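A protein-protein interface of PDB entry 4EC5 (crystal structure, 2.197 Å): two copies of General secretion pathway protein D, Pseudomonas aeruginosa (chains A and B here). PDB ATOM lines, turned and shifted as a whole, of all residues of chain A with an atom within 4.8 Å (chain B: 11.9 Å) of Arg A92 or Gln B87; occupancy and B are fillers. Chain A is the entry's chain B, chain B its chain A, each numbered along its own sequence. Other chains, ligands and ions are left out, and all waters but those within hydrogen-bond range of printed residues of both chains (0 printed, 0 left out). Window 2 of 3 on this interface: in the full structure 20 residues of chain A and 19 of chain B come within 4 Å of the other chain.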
ATOM      1  N   VAL A  47     -34.848 -20.813 -13.403  1.00  0.00           N
ATOM      2  CA  VAL A  47     -34.452 -22.173 -13.050  1.00  0.00           C
ATOM      3  C   VAL A  47     -34.255 -22.202 -11.533  1.00  0.00           C
ATOM      4  O   VAL A  47     -33.346 -21.558 -11.014  1.00  0.00           O
ATOM      5  CB  VAL A  47     -33.265 -22.674 -13.897  1.00  0.00           C
ATOM      6  CG1 VAL A  47     -33.732 -22.957 -15.328  1.00  0.00           C
ATOM      7  CG2 VAL A  47     -32.113 -21.699 -13.859  1.00  0.00           C
ATOM      8  N   VAL A  48     -35.097 -22.942 -10.823  1.00  0.00           N
ATOM      9  CA  VAL A  48     -35.127 -22.890  -9.365  1.00  0.00           C
ATOM     10  C   VAL A  48     -34.341 -24.059  -8.767  1.00  0.00           C
ATOM     11  O   VAL A  48     -34.596 -25.224  -9.078  1.00  0.00           O
ATOM     12  CB  VAL A  48     -36.588 -22.915  -8.885  1.00  0.00           C
ATOM     13  CG1 VAL A  48     -36.659 -22.774  -7.374  1.00  0.00           C
ATOM     14  CG2 VAL A  48     -37.375 -21.795  -9.560  1.00  0.00           C
ATOM     15  N   ASP A  49     -33.383 -23.727  -7.903  1.00  0.00           N
ATOM     16  CA  ASP A  49     -32.551 -24.724  -7.240  1.00  0.00           C
ATOM     17  C   ASP A  49     -33.411 -25.642  -6.373  1.00  0.00           C
ATOM     18  O   ASP A  49     -34.334 -25.181  -5.702  1.00  0.00           O
ATOM     19  CB  ASP A  49     -31.478 -24.025  -6.399  1.00  0.00           C
ATOM     20  CG  ASP A  49     -30.510 -24.992  -5.756  1.00  0.00           C
ATOM     21  OD1 ASP A  49     -30.814 -25.503  -4.655  1.00  0.00           O
ATOM     22  OD2 ASP A  49     -29.436 -25.235  -6.344  1.00  0.00           O
ATOM     23  N   PRO A  50     -33.116 -26.954  -6.392  1.00  0.00           N
ATOM     24  CA  PRO A  50     -33.918 -27.930  -5.641  1.00  0.00           C
ATOM     25  C   PRO A  50     -34.123 -27.615  -4.157  1.00  0.00           C
ATOM     26  O   PRO A  50     -35.142 -27.998  -3.583  1.00  0.00           O
ATOM     27  CB  PRO A  50     -33.158 -29.249  -5.818  1.00  0.00           C
ATOM     28  CG  PRO A  50     -32.263 -29.059  -6.986  1.00  0.00           C
ATOM     29  CD  PRO A  50     -32.064 -27.591  -7.206  1.00  0.00           C
ATOM     30  N   THR A  83     -31.248 -15.655  -3.624  1.00  0.00           N
ATOM     31  CA  THR A  83     -30.518 -14.782  -4.509  1.00  0.00           C
ATOM     32  C   THR A  83     -30.814 -15.170  -5.943  1.00  0.00           C
ATOM     33  O   THR A  83     -30.976 -16.335  -6.246  1.00  0.00           O
ATOM     34  CB  THR A  83     -29.018 -14.898  -4.264  1.00  0.00           C
ATOM     35  OG1 THR A  83     -28.716 -14.424  -2.955  1.00  0.00           O
ATOM     36  CG2 THR A  83     -28.241 -14.103  -5.262  1.00  0.00           C
ATOM     37  N   VAL A  84     -30.890 -14.182  -6.820  1.00  0.00           N
ATOM     38  CA  VAL A  84     -31.204 -14.421  -8.217  1.00  0.00           C
ATOM     39  C   VAL A  84     -29.921 -14.193  -8.985  1.00  0.00           C
ATOM     40  O   VAL A  84     -29.319 -13.119  -8.906  1.00  0.00           O
ATOM     41  CB  VAL A  84     -32.343 -13.488  -8.691  1.00  0.00           C
ATOM     42  CG1 VAL A  84     -32.669 -13.731 -10.162  1.00  0.00           C
ATOM     43  CG2 VAL A  84     -33.585 -13.658  -7.821  1.00  0.00           C
ATOM     44  N   VAL A  85     -29.506 -15.204  -9.739  1.00  0.00           N
ATOM     45  CA  VAL A  85     -28.233 -15.136 -10.429  1.00  0.00           C
ATOM     46  C   VAL A  85     -28.404 -15.268 -11.932  1.00  0.00           C
ATOM     47  O   VAL A  85     -28.987 -16.225 -12.438  1.00  0.00           O
ATOM     48  CB  VAL A  85     -27.278 -16.246  -9.923  1.00  0.00           C
ATOM     49  CG1 VAL A  85     -25.897 -16.108 -10.551  1.00  0.00           C
ATOM     50  CG2 VAL A  85     -27.200 -16.243  -8.397  1.00  0.00           C
ATOM     51  N   GLN A  87     -28.004 -16.170 -15.584  1.00  0.00           N
ATOM     52  CA  GLN A  87     -27.468 -17.281 -16.333  1.00  0.00           C
ATOM     53  C   GLN A  87     -27.879 -17.067 -17.776  1.00  0.00           C
ATOM     54  O   GLN A  87     -28.747 -17.752 -18.281  1.00  0.00           O
ATOM     55  CB  GLN A  87     -28.016 -18.603 -15.803  1.00  0.00           C
ATOM     56  N   GLN A  90     -31.891 -16.875 -19.088  1.00  0.00           N
ATOM     57  CA  GLN A  90     -32.577 -17.379 -17.910  1.00  0.00           C
ATOM     58  C   GLN A  90     -31.962 -16.805 -16.646  1.00  0.00           C
ATOM     59  O   GLN A  90     -30.900 -16.233 -16.699  1.00  0.00           O
ATOM     60  CB  GLN A  90     -32.501 -18.904 -17.876  1.00  0.00           C
ATOM     61  N   ALA A  91     -32.648 -16.932 -15.520  1.00  0.00           N
ATOM     62  CA  ALA A  91     -32.076 -16.570 -14.234  1.00  0.00           C
ATOM     63  C   ALA A  91     -32.184 -17.717 -13.235  1.00  0.00           C
ATOM     64  O   ALA A  91     -33.204 -18.368 -13.143  1.00  0.00           O
ATOM     65  CB  ALA A  91     -32.733 -15.339 -13.687  1.00  0.00           C
ATOM     66  N   ARG A  92     -31.112 -17.941 -12.485  1.00  0.00           N
ATOM     67  CA  ARG A  92     -31.039 -19.017 -11.504  1.00  0.00           C
ATOM     68  C   ARG A  92     -31.466 -18.513 -10.116  1.00  0.00           C
ATOM     69  O   ARG A  92     -30.931 -17.505  -9.653  1.00  0.00           O
ATOM     70  CB  ARG A  92     -29.588 -19.506 -11.505  1.00  0.00           C
ATOM     71  CG  ARG A  92     -29.203 -20.600 -10.528  1.00  0.00           C
ATOM     72  CD  ARG A  92     -29.933 -21.907 -10.804  1.00  0.00           C
ATOM     73  NE  ARG A  92     -29.353 -22.991 -10.015  1.00  0.00           N
ATOM     74  CZ  ARG A  92     -29.801 -24.244  -9.993  1.00  0.00           C
ATOM     75  NH1 ARG A  92     -30.824 -24.611 -10.756  1.00  0.00           N
ATOM     76  NH2 ARG A  92     -29.196 -25.142  -9.228  1.00  0.00           N
ATOM     77  N   ILE A  93     -32.398 -19.185  -9.443  1.00  0.00           N
ATOM     78  CA  ILE A  93     -32.759 -18.783  -8.076  1.00  0.00           C
ATOM     79  C   ILE A  93     -32.136 -19.770  -7.073  1.00  0.00           C
ATOM     80  O   ILE A  93     -32.394 -20.970  -7.141  1.00  0.00           O
ATOM     81  CB  ILE A  93     -34.292 -18.686  -7.903  1.00  0.00           C
ATOM     82  CG1 ILE A  93     -34.867 -17.669  -8.896  1.00  0.00           C
ATOM     83  CG2 ILE A  93     -34.642 -18.265  -6.481  1.00  0.00           C
ATOM     84  CD1 ILE A  93     -36.384 -17.542  -8.868  1.00  0.00           C
ATOM     85  N   VAL A  94     -31.325 -19.261  -6.146  1.00  0.00           N
ATOM     86  CA  VAL A  94     -30.575 -20.114  -5.216  1.00  0.00           C
ATOM     87  C   VAL A  94     -30.591 -19.577  -3.785  1.00  0.00           C
ATOM     88  O   VAL A  94     -30.697 -18.369  -3.583  1.00  0.00           O
ATOM     89  CB  VAL A  94     -29.107 -20.271  -5.660  1.00  0.00           C
ATOM     90  CG1 VAL A  94     -29.015 -21.176  -6.869  1.00  0.00           C
ATOM     91  CG2 VAL A  94     -28.498 -18.913  -5.963  1.00  0.00           C
ATOM     92  N   THR B  45     -14.617 -23.635   2.444  1.00  0.00           N
ATOM     93  CA  THR B  45     -14.222 -23.866   1.063  1.00  0.00           C
ATOM     94  C   THR B  45     -15.229 -23.257   0.097  1.00  0.00           C
ATOM     95  O   THR B  45     -16.428 -23.401   0.273  1.00  0.00           O
ATOM     96  CB  THR B  45     -14.076 -25.340   0.755  1.00  0.00           C
ATOM     97  OG1 THR B  45     -13.317 -25.963   1.790  1.00  0.00           O
ATOM     98  CG2 THR B  45     -13.359 -25.520  -0.567  1.00  0.00           C
ATOM     99  N   PHE B  46     -14.733 -22.564  -0.916  1.00  0.00           N
ATOM    100  CA  PHE B  46     -15.588 -21.840  -1.837  1.00  0.00           C
ATOM    101  C   PHE B  46     -15.384 -22.302  -3.253  1.00  0.00           C
ATOM    102  O   PHE B  46     -14.274 -22.549  -3.680  1.00  0.00           O
ATOM    103  CB  PHE B  46     -15.299 -20.345  -1.783  1.00  0.00           C
ATOM    104  CG  PHE B  46     -15.611 -19.724  -0.475  1.00  0.00           C
ATOM    105  CD1 PHE B  46     -16.910 -19.611  -0.053  1.00  0.00           C
ATOM    106  CD2 PHE B  46     -14.611 -19.264   0.340  1.00  0.00           C
ATOM    107  CE1 PHE B  46     -17.207 -19.047   1.152  1.00  0.00           C
ATOM    108  CE2 PHE B  46     -14.905 -18.696   1.546  1.00  0.00           C
ATOM    109  CZ  PHE B  46     -16.205 -18.588   1.952  1.00  0.00           C
ATOM    110  N   VAL B  47     -16.466 -22.400  -4.000  1.00  0.00           N
ATOM    111  CA  VAL B  47     -16.326 -22.584  -5.432  1.00  0.00           C
ATOM    112  C   VAL B  47     -16.502 -21.181  -6.002  1.00  0.00           C
ATOM    113  O   VAL B  47     -17.515 -20.530  -5.747  1.00  0.00           O
ATOM    114  CB  VAL B  47     -17.352 -23.573  -6.028  1.00  0.00           C
ATOM    115  CG1 VAL B  47     -17.276 -23.591  -7.544  1.00  0.00           C
ATOM    116  CG2 VAL B  47     -17.127 -24.971  -5.472  1.00  0.00           C
ATOM    117  N   VAL B  48     -15.523 -20.708  -6.765  1.00  0.00           N
ATOM    118  CA  VAL B  48     -15.578 -19.345  -7.282  1.00  0.00           C
ATOM    119  C   VAL B  48     -16.070 -19.292  -8.725  1.00  0.00           C
ATOM    120  O   VAL B  48     -15.407 -19.809  -9.622  1.00  0.00           O
ATOM    121  CB  VAL B  48     -14.187 -18.709  -7.156  1.00  0.00           C
ATOM    122  CG1 VAL B  48     -14.191 -17.303  -7.726  1.00  0.00           C
ATOM    123  CG2 VAL B  48     -13.772 -18.662  -5.694  1.00  0.00           C
ATOM    124  N   ASP B  49     -17.226 -18.675  -8.950  1.00  0.00           N
ATOM    125  CA  ASP B  49     -17.762 -18.574 -10.301  1.00  0.00           C
ATOM    126  C   ASP B  49     -16.715 -17.978 -11.239  1.00  0.00           C
ATOM    127  O   ASP B  49     -15.998 -17.052 -10.859  1.00  0.00           O
ATOM    128  CB  ASP B  49     -19.025 -17.711 -10.300  1.00  0.00           C
ATOM    129  CG  ASP B  49     -19.640 -17.580 -11.678  1.00  0.00           C
ATOM    130  OD1 ASP B  49     -19.210 -16.690 -12.438  1.00  0.00           O
ATOM    131  OD2 ASP B  49     -20.547 -18.374 -12.006  1.00  0.00           O
ATOM    132  N   PRO B  50     -16.616 -18.511 -12.467  1.00  0.00           N
ATOM    133  CA  PRO B  50     -15.644 -18.010 -13.446  1.00  0.00           C
ATOM    134  C   PRO B  50     -15.676 -16.497 -13.653  1.00  0.00           C
ATOM    135  O   PRO B  50     -14.651 -15.896 -13.971  1.00  0.00           O
ATOM    136  CB  PRO B  50     -15.971 -18.769 -14.733  1.00  0.00           C
ATOM    137  CG  PRO B  50     -16.714 -19.973 -14.298  1.00  0.00           C
ATOM    138  CD  PRO B  50     -17.352 -19.684 -12.967  1.00  0.00           C
ATOM    139  N   ARG B  51     -16.847 -15.892 -13.463  1.00  0.00           N
ATOM    140  CA  ARG B  51     -16.991 -14.458 -13.674  1.00  0.00           C
ATOM    141  C   ARG B  51     -16.427 -13.603 -12.540  1.00  0.00           C
ATOM    142  O   ARG B  51     -16.304 -12.387 -12.691  1.00  0.00           O
ATOM    143  CB  ARG B  51     -18.469 -14.096 -13.866  1.00  0.00           C
ATOM    144  CG  ARG B  51     -19.111 -14.687 -15.114  1.00  0.00           C
ATOM    145  CD  ARG B  51     -20.634 -14.561 -15.070  1.00  0.00           C
ATOM    146  NE  ARG B  51     -21.242 -15.520 -14.146  1.00  0.00           N
ATOM    147  CZ  ARG B  51     -22.549 -15.625 -13.922  1.00  0.00           C
ATOM    148  NH1 ARG B  51     -23.406 -14.832 -14.551  1.00  0.00           N
ATOM    149  NH2 ARG B  51     -23.004 -16.538 -13.072  1.00  0.00           N
ATOM    150  N   VAL B  52     -16.088 -14.215 -11.408  1.00  0.00           N
ATOM    151  CA  VAL B  52     -15.538 -13.439 -10.303  1.00  0.00           C
ATOM    152  C   VAL B  52     -14.111 -13.020 -10.649  1.00  0.00           C
ATOM    153  O   VAL B  52     -13.232 -13.870 -10.813  1.00  0.00           O
ATOM    154  CB  VAL B  52     -15.589 -14.191  -8.953  1.00  0.00           C
ATOM    155  CG1 VAL B  52     -15.011 -13.329  -7.833  1.00  0.00           C
ATOM    156  CG2 VAL B  52     -17.021 -14.599  -8.626  1.00  0.00           C
ATOM    157  N   THR B  83     -21.519 -12.110  -4.111  1.00  0.00           N
ATOM    158  CA  THR B  83     -22.239 -12.678  -2.983  1.00  0.00           C
ATOM    159  C   THR B  83     -22.028 -14.182  -2.890  1.00  0.00           C
ATOM    160  O   THR B  83     -21.700 -14.839  -3.878  1.00  0.00           O
ATOM    161  CB  THR B  83     -23.734 -12.322  -3.077  1.00  0.00           C
ATOM    162  OG1 THR B  83     -24.422 -12.813  -1.918  1.00  0.00           O
ATOM    163  CG2 THR B  83     -24.350 -12.938  -4.320  1.00  0.00           C
ATOM    164  N   VAL B  84     -22.213 -14.715  -1.689  1.00  0.00           N
ATOM    165  CA  VAL B  84     -22.060 -16.139  -1.437  1.00  0.00           C
ATOM    166  C   VAL B  84     -23.404 -16.873  -1.414  1.00  0.00           C
ATOM    167  O   VAL B  84     -24.320 -16.488  -0.687  1.00  0.00           O
ATOM    168  CB  VAL B  84     -21.300 -16.388  -0.121  1.00  0.00           C
ATOM    169  CG1 VAL B  84     -20.931 -17.852   0.022  1.00  0.00           C
ATOM    170  CG2 VAL B  84     -20.058 -15.505  -0.057  1.00  0.00           C
ATOM    171  N   VAL B  85     -23.515 -17.927  -2.221  1.00  0.00           N
ATOM    172  CA  VAL B  85     -24.749 -18.704  -2.317  1.00  0.00           C
ATOM    173  C   VAL B  85     -24.479 -20.192  -2.107  1.00  0.00           C
ATOM    174  O   VAL B  85     -23.333 -20.635  -2.163  1.00  0.00           O
ATOM    175  CB  VAL B  85     -25.433 -18.494  -3.686  1.00  0.00           C
ATOM    176  CG1 VAL B  85     -25.673 -17.017  -3.955  1.00  0.00           C
ATOM    177  CG2 VAL B  85     -24.600 -19.118  -4.803  1.00  0.00           C
ATOM    178  N   ALA B  86     -25.539 -20.958  -1.911  1.00  0.00           N
ATOM    179  CA  ALA B  86     -25.410 -22.395  -1.827  1.00  0.00           C
ATOM    180  C   ALA B  86     -25.889 -23.035  -3.126  1.00  0.00           C
ATOM    181  O   ALA B  86     -27.056 -22.926  -3.483  1.00  0.00           O
ATOM    182  CB  ALA B  86     -26.211 -22.907  -0.676  1.00  0.00           C
ATOM    183  N   GLN B  87     -24.989 -23.687  -3.843  1.00  0.00           N
ATOM    184  CA  GLN B  87     -25.374 -24.479  -4.992  1.00  0.00           C
ATOM    185  C   GLN B  87     -24.690 -25.840  -4.967  1.00  0.00           C
ATOM    186  O   GLN B  87     -23.490 -25.926  -4.757  1.00  0.00           O
ATOM    187  CB  GLN B  87     -25.006 -23.760  -6.277  1.00  0.00           C
ATOM    188  CG  GLN B  87     -26.161 -23.293  -7.109  1.00  0.00           C
ATOM    189  CD  GLN B  87     -25.699 -22.788  -8.445  1.00  0.00           C
ATOM    190  OE1 GLN B  87     -25.513 -21.596  -8.641  1.00  0.00           O
ATOM    191  NE2 GLN B  87     -25.482 -23.701  -9.369  1.00  0.00           N
ATOM    192  N   GLY B  88     -25.440 -26.900  -5.208  1.00  0.00           N
ATOM    193  CA  GLY B  88     -24.856 -28.218  -5.351  1.00  0.00           C
ATOM    194  C   GLY B  88     -24.035 -28.694  -4.172  1.00  0.00           C
ATOM    195  O   GLY B  88     -23.001 -29.328  -4.350  1.00  0.00           O
ATOM    196  N   ASP B  89     -24.486 -28.387  -2.965  1.00  0.00           N
ATOM    197  CA  ASP B  89     -23.807 -28.898  -1.762  1.00  0.00           C
ATOM    198  C   ASP B  89     -22.476 -28.199  -1.511  1.00  0.00           C
ATOM    199  O   ASP B  89     -21.642 -28.702  -0.766  1.00  0.00           O
ATOM    200  CB  ASP B  89     -23.557 -30.395  -1.912  1.00  0.00           C
ATOM    201  N   GLN B  90     -22.269 -27.051  -2.148  1.00  0.00           N
ATOM    202  CA  GLN B  90     -21.039 -26.293  -1.971  1.00  0.00           C
ATOM    203  C   GLN B  90     -21.350 -24.813  -1.893  1.00  0.00           C
ATOM    204  O   GLN B  90     -22.342 -24.362  -2.436  1.00  0.00           O
ATOM    205  CB  GLN B  90     -20.076 -26.566  -3.121  1.00  0.00           C
ATOM    206  N   ALA B  91     -20.497 -24.062  -1.213  1.00  0.00           N
ATOM    207  CA  ALA B  91     -20.663 -22.627  -1.118  1.00  0.00           C
ATOM    208  C   ALA B  91     -20.045 -21.974  -2.326  1.00  0.00           C
ATOM    209  O   ALA B  91     -18.908 -22.250  -2.678  1.00  0.00           O
ATOM    210  CB  ALA B  91     -20.038 -22.108   0.131  1.00  0.00           C
ATOM    211  N   ARG B  92     -20.810 -21.098  -2.956  1.00  0.00           N
ATOM    212  CA  ARG B  92     -20.424 -20.531  -4.224  1.00  0.00           C
ATOM    213  C   ARG B  92     -20.403 -19.010  -4.221  1.00  0.00           C
ATOM    214  O   ARG B  92     -21.331 -18.381  -3.757  1.00  0.00           O
ATOM    215  CB  ARG B  92     -21.396 -21.038  -5.274  1.00  0.00           C
ATOM    216  CG  ARG B  92     -20.910 -20.939  -6.683  1.00  0.00           C
ATOM    217  CD  ARG B  92     -21.399 -22.098  -7.476  1.00  0.00           C
ATOM    218  NE  ARG B  92     -20.687 -22.169  -8.743  1.00  0.00           N
ATOM    219  CZ  ARG B  92     -21.009 -21.432  -9.790  1.00  0.00           C
ATOM    220  NH1 ARG B  92     -22.039 -20.603  -9.705  1.00  0.00           N
ATOM    221  NH2 ARG B  92     -20.322 -21.529 -10.911  1.00  0.00           N
ATOM    222  N   ILE B  93     -19.339 -18.426  -4.748  1.00  0.00           N
ATOM    223  CA  ILE B  93     -19.251 -16.978  -4.884  1.00  0.00           C
ATOM    224  C   ILE B  93     -19.673 -16.611  -6.308  1.00  0.00           C
ATOM    225  O   ILE B  93     -19.099 -17.107  -7.279  1.00  0.00           O
ATOM    226  CB  ILE B  93     -17.826 -16.487  -4.567  1.00  0.00           C
ATOM    227  CG1 ILE B  93     -17.443 -16.880  -3.135  1.00  0.00           C
ATOM    228  CG2 ILE B  93     -17.724 -14.981  -4.776  1.00  0.00           C
ATOM    229  CD1 ILE B  93     -16.014 -16.547  -2.754  1.00  0.00           C
ATOM    230  N   VAL B  94     -20.670 -15.738  -6.423  1.00  0.00           N
ATOM    231  CA  VAL B  94     -21.270 -15.404  -7.715  1.00  0.00           C
ATOM    232  C   VAL B  94     -21.481 -13.897  -7.836  1.00  0.00           C
ATOM    233  O   VAL B  94     -21.645 -13.212  -6.828  1.00  0.00           O
ATOM    234  CB  VAL B  94     -22.608 -16.134  -7.911  1.00  0.00           C
ATOM    235  CG1 VAL B  94     -22.363 -17.609  -8.197  1.00  0.00           C
ATOM    236  CG2 VAL B  94     -23.487 -15.961  -6.687  1.00  0.00           C
ATOM    237  N   PRO B  95     -21.482 -13.371  -9.071  1.00  0.00           N
ATOM    238  CA  PRO B  95     -21.789 -11.941  -9.209  1.00  0.00           C
ATOM    239  C   PRO B  95     -23.209 -11.557  -8.807  1.00  0.00           C
ATOM    240  O   PRO B  95     -24.177 -12.243  -9.137  1.00  0.00           O
ATOM    241  CB  PRO B  95     -21.530 -11.655 -10.699  1.00  0.00           C
ATOM    242  CG  PRO B  95     -20.943 -12.904 -11.281  1.00  0.00           C
ATOM    243  CD  PRO B  95     -21.313 -14.032 -10.375  1.00  0.00           C
ATOM    244  N   ASN B  96     -23.310 -10.442  -8.092  1.00  0.00           N
ATOM    245  CA  ASN B  96     -24.585  -9.923  -7.629  1.00  0.00           C
ATOM    246  C   ASN B  96     -25.143  -9.002  -8.705  1.00  0.00           C
ATOM    247  O   ASN B  96     -24.389  -8.475  -9.525  1.00  0.00           O
ATOM    248  CB  ASN B  96     -24.406  -9.163  -6.313  1.00  0.00           C
ATOM    249  CG  ASN B  96     -25.668  -9.143  -5.473  1.00  0.00           C
ATOM    250  OD1 ASN B  96     -26.779  -9.082  -6.000  1.00  0.00           O
ATOM    251  ND2 ASN B  96     -25.502  -9.205  -4.155  1.00  0.00           N
ATOM    252  N   ALA B  97     -26.457  -8.807  -8.713  1.00  0.00           N
ATOM    253  CA  ALA B  97     -27.074  -7.928  -9.696  1.00  0.00           C
ATOM    254  C   ALA B  97     -26.809  -6.472  -9.329  1.00  0.00           C
ATOM    255  O   ALA B  97     -27.219  -5.558 -10.043  1.00  0.00           O
ATOM    256  CB  ALA B  97     -28.564  -8.182  -9.752  1.00  0.00           C
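Among the printed residues, pairs that only touch across the chains: Asp A49 with Gln B87, Thr A83 with Val B85, Val A85 with Arg B51, Arg A92 with Gln B87, Val A94 with Val B85, Val A94 with Ala B86 and Val A94 with Gln B87.
Printed residues of chain B that touch a printed residue of chain A: Arg B51, Val B85, Ala B86 and Gln B87.
Hydrophobic or aromatic side chains of chain B that line the printed part of chain A: Val B85.
Hydrophobic or aromatic side chains of chain A that line the printed part of chain B: Val A85 and Val A94.
Along chain A the printed residues that touch a printed residue of chain B span positions 49 to 94.
Among the printed residues, no Asp or Glu carboxylate lies within 4 Å of a Lys or Arg side-chain nitrogen of the other chain.
The backbone NH (N) of Val A85 sits at hydrogen-bond distance from the backbone carbonyl oxygen (O) of Arg A92.
The backbone carbonyl oxygen (O) of Val A94 is in hydrogen-bond range of the backbone NH (N) of Thr A83.
N of Arg B92 lies within hydrogen-bond range of O of Val B85, at 2.7 Å.
The guanidinium group of Arg B51 lies within salt-bridge range of the side-chain carboxylate of Asp B49 (2.9 Å).
The side-chain carboxylate of Asp A49 lies within salt-bridge range of the guanidinium group of Arg A92, 2.9 Å away.
The backbone NH of Asp A49 sits at hydrogen-bond distance from the backbone carbonyl oxygen of Ile A93.
Printed residues of chain B within 4 Å of Arg A92: Gln B87.
Printed residues of chain A within 4 Å of Gln B87: Asp A49, Arg A92 and Val A94.
No residue of chain B comes within 4 Å of Val A47.
Asp A49 touches one residue of chain B.
Thr A83 touches just one residue of chain B: Val B85 (3.97 Å).
No residue of chain B comes within 4 Å of Val A84.
Of chain B, only Arg B51 comes within 4 Å of Val A85.
No residue of chain B comes within 4 Å of Gln A87.
No residue of chain B comes within 4 Å of Ile A93.
Of the printed residues of chain A, Val B85 touches Thr A83 and Val A94.
Of the printed residues of chain B, Val A94 touches Val B85 (3.8 Å), Ala B86 (3.999 Å) and Gln B87 (3.6 Å).
Printed residues of chain A within 4 Å of Ala B86: Val A94.
Printed residues of chain A within 4 Å of Arg B51: Val A85 (3.9 Å).
The nearest printed residue of chain A that does not touch Ala B86 is Asp A49 (4.4 Å).
Asp A49 touches Gln B87, but with the chains exchanged Gln A87 does not touch Asp B49 (8.2 Å).
Thr A83 touches Val B85, but with the chains exchanged Val A85 does not touch Thr B83 (6.0 Å).
Arg A92 touches Gln B87, but with the chains exchanged Gln A87 does not touch Arg B92 (8.8 Å).
Val A94 touches Gln B87, but with the chains exchanged Gln A87 does not touch Val B94 (9.4 Å).
Positions printed for both chains: 47, 48, 49, 50, 83, 84, 85, 87, 90, 91, 92, 93 and 94.
Of the 7 pairs that touch across the chains among the printed residues, none has its exchanged pair printed and touching as well.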
